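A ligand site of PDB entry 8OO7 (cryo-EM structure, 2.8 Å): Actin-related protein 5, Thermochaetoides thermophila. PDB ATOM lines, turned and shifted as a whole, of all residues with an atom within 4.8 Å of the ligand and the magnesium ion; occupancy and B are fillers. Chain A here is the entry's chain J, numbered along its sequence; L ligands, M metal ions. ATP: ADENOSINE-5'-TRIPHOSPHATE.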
ATOM      1  N   ASP A  62      20.673   5.527  -9.914  1.00  0.00           N
ATOM      2  CA  ASP A  62      20.770   4.884  -8.609  1.00  0.00           C
ATOM      3  C   ASP A  62      19.380   4.458  -8.128  1.00  0.00           C
ATOM      4  O   ASP A  62      18.550   5.308  -7.807  1.00  0.00           O
ATOM      5  CB  ASP A  62      21.447   5.809  -7.603  1.00  0.00           C
ATOM      6  CG  ASP A  62      21.586   5.179  -6.232  1.00  0.00           C
ATOM      7  OD1 ASP A  62      21.672   3.946  -6.144  1.00  0.00           O
ATOM      8  OD2 ASP A  62      21.610   5.941  -5.241  1.00  0.00           O
ATOM      9  N   ASN A  63      19.151   3.151  -8.084  1.00  0.00           N
ATOM     10  CA  ASN A  63      17.907   2.540  -7.631  1.00  0.00           C
ATOM     11  C   ASN A  63      17.664   2.618  -6.130  1.00  0.00           C
ATOM     12  O   ASN A  63      17.517   1.591  -5.477  1.00  0.00           O
ATOM     13  CB  ASN A  63      17.846   1.065  -8.047  1.00  0.00           C
ATOM     14  CG  ASN A  63      17.166   0.860  -9.376  1.00  0.00           C
ATOM     15  OD1 ASN A  63      16.067   1.357  -9.612  1.00  0.00           O
ATOM     16  ND2 ASN A  63      17.802   0.096 -10.252  1.00  0.00           N
ATOM     17  N   GLY A  64      17.601   3.825  -5.579  1.00  0.00           N
ATOM     18  CA  GLY A  64      17.266   3.963  -4.174  1.00  0.00           C
ATOM     19  C   GLY A  64      15.805   3.643  -3.937  1.00  0.00           C
ATOM     20  O   GLY A  64      14.922   4.246  -4.553  1.00  0.00           O
ATOM     21  N   SER A  65      15.540   2.671  -3.057  1.00  0.00           N
ATOM     22  CA  SER A  65      14.176   2.387  -2.616  1.00  0.00           C
ATOM     23  C   SER A  65      13.513   3.593  -1.973  1.00  0.00           C
ATOM     24  O   SER A  65      12.279   3.690  -1.959  1.00  0.00           O
ATOM     25  CB  SER A  65      14.173   1.216  -1.630  1.00  0.00           C
ATOM     26  OG  SER A  65      14.899   0.117  -2.147  1.00  0.00           O
ATOM     27  N   HIS A  66      14.295   4.516  -1.417  1.00  0.00           N
ATOM     28  CA  HIS A  66      13.784   5.808  -0.996  1.00  0.00           C
ATOM     29  C   HIS A  66      13.816   6.857  -2.106  1.00  0.00           C
ATOM     30  O   HIS A  66      12.923   7.706  -2.155  1.00  0.00           O
ATOM     31  CB  HIS A  66      14.562   6.309   0.219  1.00  0.00           C
ATOM     32  CG  HIS A  66      14.218   7.698   0.639  1.00  0.00           C
ATOM     33  ND1 HIS A  66      13.074   8.007   1.340  1.00  0.00           N
ATOM     34  CD2 HIS A  66      14.887   8.871   0.492  1.00  0.00           C
ATOM     35  CE1 HIS A  66      13.038   9.293   1.586  1.00  0.00           C
ATOM     36  NE2 HIS A  66      14.122   9.850   1.088  1.00  0.00           N
ATOM     37  N   SER A  67      14.805   6.817  -2.989  1.00  0.00           N
ATOM     38  CA  SER A  67      14.920   7.839  -4.025  1.00  0.00           C
ATOM     39  C   SER A  67      15.659   7.246  -5.214  1.00  0.00           C
ATOM     40  O   SER A  67      16.832   6.880  -5.096  1.00  0.00           O
ATOM     41  CB  SER A  67      15.646   9.079  -3.507  1.00  0.00           C
ATOM     42  OG  SER A  67      15.647  10.117  -4.473  1.00  0.00           O
ATOM     43  N   ARG A  69      17.694   8.137  -8.151  1.00  0.00           N
ATOM     44  CA  ARG A  69      18.520   9.256  -8.586  1.00  0.00           C
ATOM     45  C   ARG A  69      19.073   8.960  -9.983  1.00  0.00           C
ATOM     46  O   ARG A  69      19.622   7.887 -10.217  1.00  0.00           O
ATOM     47  CB  ARG A  69      19.648   9.490  -7.595  1.00  0.00           C
ATOM     48  CG  ARG A  69      19.144  10.029  -6.273  1.00  0.00           C
ATOM     49  CD  ARG A  69      20.104   9.740  -5.153  1.00  0.00           C
ATOM     50  NE  ARG A  69      20.118   8.299  -4.877  1.00  0.00           N
ATOM     51  CZ  ARG A  69      19.755   7.761  -3.721  1.00  0.00           C
ATOM     52  NH1 ARG A  69      19.333   8.501  -2.715  1.00  0.00           N
ATOM     53  NH2 ARG A  69      19.801   6.439  -3.588  1.00  0.00           N
ATOM     54  N   GLY A 124      15.343  -4.232  -0.470  1.00  0.00           N
ATOM     55  CA  GLY A 124      16.064  -3.494  -1.480  1.00  0.00           C
ATOM     56  C   GLY A 124      15.784  -3.947  -2.886  1.00  0.00           C
ATOM     57  O   GLY A 124      16.411  -3.454  -3.825  1.00  0.00           O
ATOM     58  N   ASP A 190      25.526   0.136  -4.781  1.00  0.00           N
ATOM     59  CA  ASP A 190      25.528   1.563  -4.442  1.00  0.00           C
ATOM     60  C   ASP A 190      26.546   1.916  -3.368  1.00  0.00           C
ATOM     61  O   ASP A 190      27.192   2.965  -3.442  1.00  0.00           O
ATOM     62  CB  ASP A 190      24.120   1.998  -4.034  1.00  0.00           C
ATOM     63  CG  ASP A 190      23.678   1.434  -2.676  1.00  0.00           C
ATOM     64  OD1 ASP A 190      24.236   0.399  -2.244  1.00  0.00           O
ATOM     65  OD2 ASP A 190      22.763   2.016  -2.053  1.00  0.00           O
ATOM     66  N   SER A 208      23.990   1.977   5.937  1.00  0.00           N
ATOM     67  CA  SER A 208      22.618   1.934   6.396  1.00  0.00           C
ATOM     68  C   SER A 208      21.768   2.780   5.467  1.00  0.00           C
ATOM     69  O   SER A 208      22.004   3.983   5.315  1.00  0.00           O
ATOM     70  CB  SER A 208      22.484   2.423   7.841  1.00  0.00           C
ATOM     71  OG  SER A 208      23.209   1.584   8.725  1.00  0.00           O
ATOM     72  N   SER A 209      20.780   2.135   4.849  1.00  0.00           N
ATOM     73  CA  SER A 209      19.980   2.780   3.818  1.00  0.00           C
ATOM     74  C   SER A 209      18.503   2.661   4.178  1.00  0.00           C
ATOM     75  O   SER A 209      18.162   2.356   5.321  1.00  0.00           O
ATOM     76  CB  SER A 209      20.270   2.151   2.459  1.00  0.00           C
ATOM     77  OG  SER A 209      19.802   0.809   2.395  1.00  0.00           O
ATOM     78  N   TYR A 210      17.625   2.914   3.209  1.00  0.00           N
ATOM     79  CA  TYR A 210      16.207   2.687   3.418  1.00  0.00           C
ATOM     80  C   TYR A 210      15.921   1.202   3.626  1.00  0.00           C
ATOM     81  O   TYR A 210      15.173   0.817   4.533  1.00  0.00           O
ATOM     82  CB  TYR A 210      15.429   3.231   2.219  1.00  0.00           C
ATOM     83  CG  TYR A 210      13.980   3.553   2.465  1.00  0.00           C
ATOM     84  CD1 TYR A 210      13.610   4.628   3.260  1.00  0.00           C
ATOM     85  CD2 TYR A 210      12.977   2.793   1.888  1.00  0.00           C
ATOM     86  CE1 TYR A 210      12.276   4.914   3.493  1.00  0.00           C
ATOM     87  CE2 TYR A 210      11.646   3.081   2.096  1.00  0.00           C
ATOM     88  CZ  TYR A 210      11.303   4.135   2.905  1.00  0.00           C
ATOM     89  OH  TYR A 210       9.968   4.429   3.101  1.00  0.00           O
ATOM     90  N   SER A 211      16.507   0.349   2.790  1.00  0.00           N
ATOM     91  CA  SER A 211      16.084  -1.049   2.766  1.00  0.00           C
ATOM     92  C   SER A 211      16.669  -1.862   3.912  1.00  0.00           C
ATOM     93  O   SER A 211      15.997  -2.751   4.444  1.00  0.00           O
ATOM     94  CB  SER A 211      16.465  -1.684   1.431  1.00  0.00           C
ATOM     95  OG  SER A 211      17.843  -1.527   1.154  1.00  0.00           O
ATOM     96  N   ALA A 212      17.900  -1.579   4.305  1.00  0.00           N
ATOM     97  CA  ALA A 212      18.697  -2.558   5.035  1.00  0.00           C
ATOM     98  C   ALA A 212      19.937  -1.870   5.589  1.00  0.00           C
ATOM     99  O   ALA A 212      20.157  -0.680   5.387  1.00  0.00           O
ATOM    100  CB  ALA A 212      19.074  -3.738   4.131  1.00  0.00           C
ATOM    101  N   GLY A 235      16.252   2.708   7.266  1.00  0.00           N
ATOM    102  CA  GLY A 235      15.461   3.903   7.474  1.00  0.00           C
ATOM    103  C   GLY A 235      13.968   3.695   7.293  1.00  0.00           C
ATOM    104  O   GLY A 235      13.166   4.430   7.868  1.00  0.00           O
ATOM    105  N   TRP A 236      13.575   2.726   6.473  1.00  0.00           N
ATOM    106  CA  TRP A 236      12.164   2.370   6.367  1.00  0.00           C
ATOM    107  C   TRP A 236      11.648   1.799   7.672  1.00  0.00           C
ATOM    108  O   TRP A 236      10.616   2.227   8.197  1.00  0.00           O
ATOM    109  CB  TRP A 236      11.961   1.354   5.243  1.00  0.00           C
ATOM    110  CG  TRP A 236      10.528   0.964   5.038  1.00  0.00           C
ATOM    111  CD1 TRP A 236       9.576   1.686   4.403  1.00  0.00           C
ATOM    112  CD2 TRP A 236       9.877  -0.212   5.552  1.00  0.00           C
ATOM    113  NE1 TRP A 236       8.375   1.014   4.446  1.00  0.00           N
ATOM    114  CE2 TRP A 236       8.540  -0.147   5.145  1.00  0.00           C
ATOM    115  CE3 TRP A 236      10.307  -1.307   6.300  1.00  0.00           C
ATOM    116  CZ2 TRP A 236       7.612  -1.136   5.462  1.00  0.00           C
ATOM    117  CZ3 TRP A 236       9.395  -2.299   6.611  1.00  0.00           C
ATOM    118  CH2 TRP A 236       8.065  -2.201   6.192  1.00  0.00           C
ATOM    119  N   GLU A 264       8.875   9.306   9.330  1.00  0.00           N
ATOM    120  CA  GLU A 264      10.136   9.383   8.599  1.00  0.00           C
ATOM    121  C   GLU A 264      10.820  10.737   8.752  1.00  0.00           C
ATOM    122  O   GLU A 264      12.054  10.802   8.855  1.00  0.00           O
ATOM    123  CB  GLU A 264       9.888   9.066   7.124  1.00  0.00           C
ATOM    124  CG  GLU A 264      11.131   8.931   6.267  1.00  0.00           C
ATOM    125  CD  GLU A 264      11.402  10.180   5.457  1.00  0.00           C
ATOM    126  OE1 GLU A 264      10.434  10.912   5.149  1.00  0.00           O
ATOM    127  OE2 GLU A 264      12.584  10.437   5.137  1.00  0.00           O
ATOM    128  N   ARG A 268      14.327  11.541  11.153  1.00  0.00           N
ATOM    129  CA  ARG A 268      15.386  12.422  10.644  1.00  0.00           C
ATOM    130  C   ARG A 268      15.675  13.593  11.575  1.00  0.00           C
ATOM    131  O   ARG A 268      16.831  13.831  11.955  1.00  0.00           O
ATOM    132  CB  ARG A 268      15.043  12.903   9.238  1.00  0.00           C
ATOM    133  CG  ARG A 268      15.277  11.831   8.188  1.00  0.00           C
ATOM    134  CD  ARG A 268      15.297  12.365   6.769  1.00  0.00           C
ATOM    135  NE  ARG A 268      13.989  12.347   6.126  1.00  0.00           N
ATOM    136  CZ  ARG A 268      13.405  13.412   5.586  1.00  0.00           C
ATOM    137  NH1 ARG A 268      13.930  14.620   5.707  1.00  0.00           N
ATOM    138  NH2 ARG A 268      12.262  13.261   4.940  1.00  0.00           N
ATOM    139  N   GLY A 690      25.352   5.813   3.066  1.00  0.00           N
ATOM    140  CA  GLY A 690      23.895   5.799   3.093  1.00  0.00           C
ATOM    141  C   GLY A 690      23.251   6.716   4.117  1.00  0.00           C
ATOM    142  O   GLY A 690      23.843   7.023   5.156  1.00  0.00           O
ATOM    143  N   GLY A 691      22.045   7.168   3.790  1.00  0.00           N
ATOM    144  CA  GLY A 691      21.418   8.238   4.562  1.00  0.00           C
ATOM    145  C   GLY A 691      21.137   7.865   6.004  1.00  0.00           C
ATOM    146  O   GLY A 691      21.278   8.687   6.902  1.00  0.00           O
ATOM    147  N   ASN A 692      20.739   6.613   6.244  1.00  0.00           N
ATOM    148  CA  ASN A 692      20.382   6.153   7.581  1.00  0.00           C
ATOM    149  C   ASN A 692      21.579   6.036   8.531  1.00  0.00           C
ATOM    150  O   ASN A 692      21.391   5.689   9.694  1.00  0.00           O
ATOM    151  CB  ASN A 692      19.659   4.807   7.452  1.00  0.00           C
ATOM    152  CG  ASN A 692      19.119   4.299   8.779  1.00  0.00           C
ATOM    153  OD1 ASN A 692      19.479   3.222   9.224  1.00  0.00           O
ATOM    154  ND2 ASN A 692      18.247   5.084   9.393  1.00  0.00           N
ATOM    155  N   LEU A 694      23.282   8.871   9.095  1.00  0.00           N
ATOM    156  CA  LEU A 694      23.521  10.273   9.393  1.00  0.00           C
ATOM    157  C   LEU A 694      23.062  10.696  10.794  1.00  0.00           C
ATOM    158  O   LEU A 694      22.997  11.896  11.065  1.00  0.00           O
ATOM    159  CB  LEU A 694      22.839  11.162   8.348  1.00  0.00           C
ATOM    160  CG  LEU A 694      23.445  11.118   6.946  1.00  0.00           C
ATOM    161  CD1 LEU A 694      22.546  11.821   5.942  1.00  0.00           C
ATOM    162  CD2 LEU A 694      24.837  11.742   6.956  1.00  0.00           C
ATOM    163  N   PHE A 695      22.738   9.751  11.674  1.00  0.00           N
ATOM    164  CA  PHE A 695      22.429  10.091  13.059  1.00  0.00           C
ATOM    165  C   PHE A 695      23.645  10.683  13.763  1.00  0.00           C
ATOM    166  O   PHE A 695      24.780  10.270  13.545  1.00  0.00           O
ATOM    167  CB  PHE A 695      21.947   8.863  13.810  1.00  0.00           C
ATOM    168  CG  PHE A 695      20.665   8.299  13.287  1.00  0.00           C
ATOM    169  CD1 PHE A 695      19.493   9.028  13.379  1.00  0.00           C
ATOM    170  CD2 PHE A 695      20.635   7.049  12.713  1.00  0.00           C
ATOM    171  CE1 PHE A 695      18.317   8.516  12.894  1.00  0.00           C
ATOM    172  CE2 PHE A 695      19.462   6.529  12.223  1.00  0.00           C
ATOM    173  CZ  PHE A 695      18.296   7.265  12.325  1.00  0.00           C
ATOM    174  N   ILE A 725      24.300  10.594   1.066  1.00  0.00           N
ATOM    175  CA  ILE A 725      23.224  10.194   0.161  1.00  0.00           C
ATOM    176  C   ILE A 725      23.638  10.196  -1.311  1.00  0.00           C
ATOM    177  O   ILE A 725      23.615   9.155  -1.969  1.00  0.00           O
ATOM    178  CB  ILE A 725      21.981  11.073   0.387  1.00  0.00           C
ATOM    179  CG1 ILE A 725      22.340  12.563   0.401  1.00  0.00           C
ATOM    180  CG2 ILE A 725      21.293  10.685   1.688  1.00  0.00           C
ATOM    181  CD1 ILE A 725      21.210  13.473  -0.022  1.00  0.00           C
HETATM  182  PG  ATP L   1      18.420   1.439  -0.853  1.00  0.00           P
HETATM  183  O1G ATP L   1      19.844   1.409  -1.281  1.00  0.00           O
HETATM  184  O2G ATP L   1      17.457   0.875  -1.906  1.00  0.00           O
HETATM  185  O3G ATP L   1      18.181   0.757   0.480  1.00  0.00           O
HETATM  186  PB  ATP L   1      18.440   4.396  -0.840  1.00  0.00           P
HETATM  187  O1B ATP L   1      19.606   4.442  -1.742  1.00  0.00           O
HETATM  188  O2B ATP L   1      17.252   5.252  -1.287  1.00  0.00           O
HETATM  189  O3B ATP L   1      17.925   2.934  -0.644  1.00  0.00           O
HETATM  190  PA  ATP L   1      19.561   6.011   1.351  1.00  0.00           P
HETATM  191  O1A ATP L   1      20.966   5.636   1.607  1.00  0.00           O
HETATM  192  O2A ATP L   1      19.348   7.280   0.523  1.00  0.00           O
HETATM  193  O3A ATP L   1      18.776   4.835   0.646  1.00  0.00           O
HETATM  194  O5' ATP L   1      18.765   6.175   2.701  1.00  0.00           O
HETATM  195  C5' ATP L   1      17.656   7.086   2.808  1.00  0.00           C
HETATM  196  C4' ATP L   1      17.123   7.002   4.224  1.00  0.00           C
HETATM  197  O4' ATP L   1      17.915   7.849   5.082  1.00  0.00           O
HETATM  198  C3' ATP L   1      15.663   7.435   4.396  1.00  0.00           C
HETATM  199  O3' ATP L   1      14.988   6.576   5.310  1.00  0.00           O
HETATM  200  C2' ATP L   1      15.797   8.852   4.956  1.00  0.00           C
HETATM  201  O2' ATP L   1      14.680   9.204   5.767  1.00  0.00           O
HETATM  202  C1' ATP L   1      17.056   8.707   5.807  1.00  0.00           C
HETATM  203  N9  ATP L   1      17.763   9.965   6.055  1.00  0.00           N
HETATM  204  C8  ATP L   1      17.985  10.974   5.149  1.00  0.00           C
HETATM  205  N7  ATP L   1      18.648  11.995   5.651  1.00  0.00           N
HETATM  206  C5  ATP L   1      18.868  11.629   6.971  1.00  0.00           C
HETATM  207  C6  ATP L   1      19.512  12.274   8.044  1.00  0.00           C
HETATM  208  N6  ATP L   1      20.076  13.473   7.953  1.00  0.00           N
HETATM  209  N1  ATP L   1      19.554  11.632   9.230  1.00  0.00           N
HETATM  210  C2  ATP L   1      18.998  10.419   9.328  1.00  0.00           C
HETATM  211  N3  ATP L   1      18.358   9.717   8.398  1.00  0.00           N
HETATM  212  C4  ATP L   1      18.327  10.375   7.233  1.00  0.00           C
HETATM  213 MG    MG M   1      20.846   2.870  -1.428  1.00  0.00          MG
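O3G of the ligand sits at hydrogen-bond distance from N of Ser 211 (2.9 Å). O3G of the ligand is in hydrogen-bond range of OG of Ser 211, at 2.4 Å. The side-chain hydroxyl (OG) of Ser 209 sits at hydrogen-bond distance from an oxygen (O3G) of the ligand. OE2 of Glu 264 is in hydrogen-bond range of O2' of the ligand (2.5 Å). N of Ser 65 lies within hydrogen-bond range of O2G of the ligand (2.9 Å). OG of Ser 65 sits at hydrogen-bond distance from O2G of the ligand (2.7 Å). The guanidinium group (NH1) of Arg 69 lies within salt-bridge range of an oxygen (O2A) of the ligand, at 3.5 Å. An oxygen (O1A) of the ligand is in hydrogen-bond range of the backbone NH of Gly 691, 2.9 Å away. O2B of the ligand is in hydrogen-bond range of N of His 66 (3.0 Å). The backbone NH (N) of Tyr 210 lies within hydrogen-bond range of an oxygen (O3A) of the ligand (3.4 Å). The guanidinium group (NE) of Arg 268 sits at hydrogen-bond distance from an oxygen (O2') of the ligand (3.2 Å). The backbone NH (N) of Asn 692 sits at hydrogen-bond distance from an oxygen (O4') of the ligand (3.3 Å). An oxygen (O2B) of the ligand is in hydrogen-bond range of the backbone NH (N) of Ser 67 (3.4 Å).
OG of Ser 209 lies within hydrogen-bond range of OG of Ser 211 (3.3 Å). N of Gly 235 sits at hydrogen-bond distance from O of Ser 209 (2.7 Å). OG of Ser 209 lies within hydrogen-bond range of O of Ala 212, at 3.4 Å. OE2 of Glu 264 lies within salt-bridge range of NE of Arg 268, at 2.6 Å. The guanidinium group (NH2) of Arg 69 lies close to the backbone carbonyl oxygen (O) of Ser 67 (3.4 Å). The side-chain carboxylate of Asp 62 is in salt-bridge range of the guanidinium group of Arg 69, at 2.5 Å. The backbone NH of Gly 235 lies within hydrogen-bond range of the backbone carbonyl oxygen of Tyr 210 (3.5 Å). O of Tyr 210 sits at hydrogen-bond distance from N of Trp 236 (3.2 Å).
Residues that only touch the ligand: Asn 63, Gly 64, Gly 235, Gly 690 and Leu 694. Hydrophobic or aromatic side chains within 4 Å of the ligand: His 66, Tyr 210 and Leu 694. Of the 24 residues printed, 17 come within 4 Å of the ligand.
Ser 209 touches the magnesium ion (CB to MG, 3.99 Å). Two residues have an atom within 4 Å of the magnesium ion: Asp 190 and Ser 209.
O1G of the ligand is bound to the magnesium ion, 1.8 Å away. The magnesium ion is bound by O1B of the ligand, 2.0 Å away. The magnesium ion is bound by OD2 of Asp 190 (2.2 Å).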
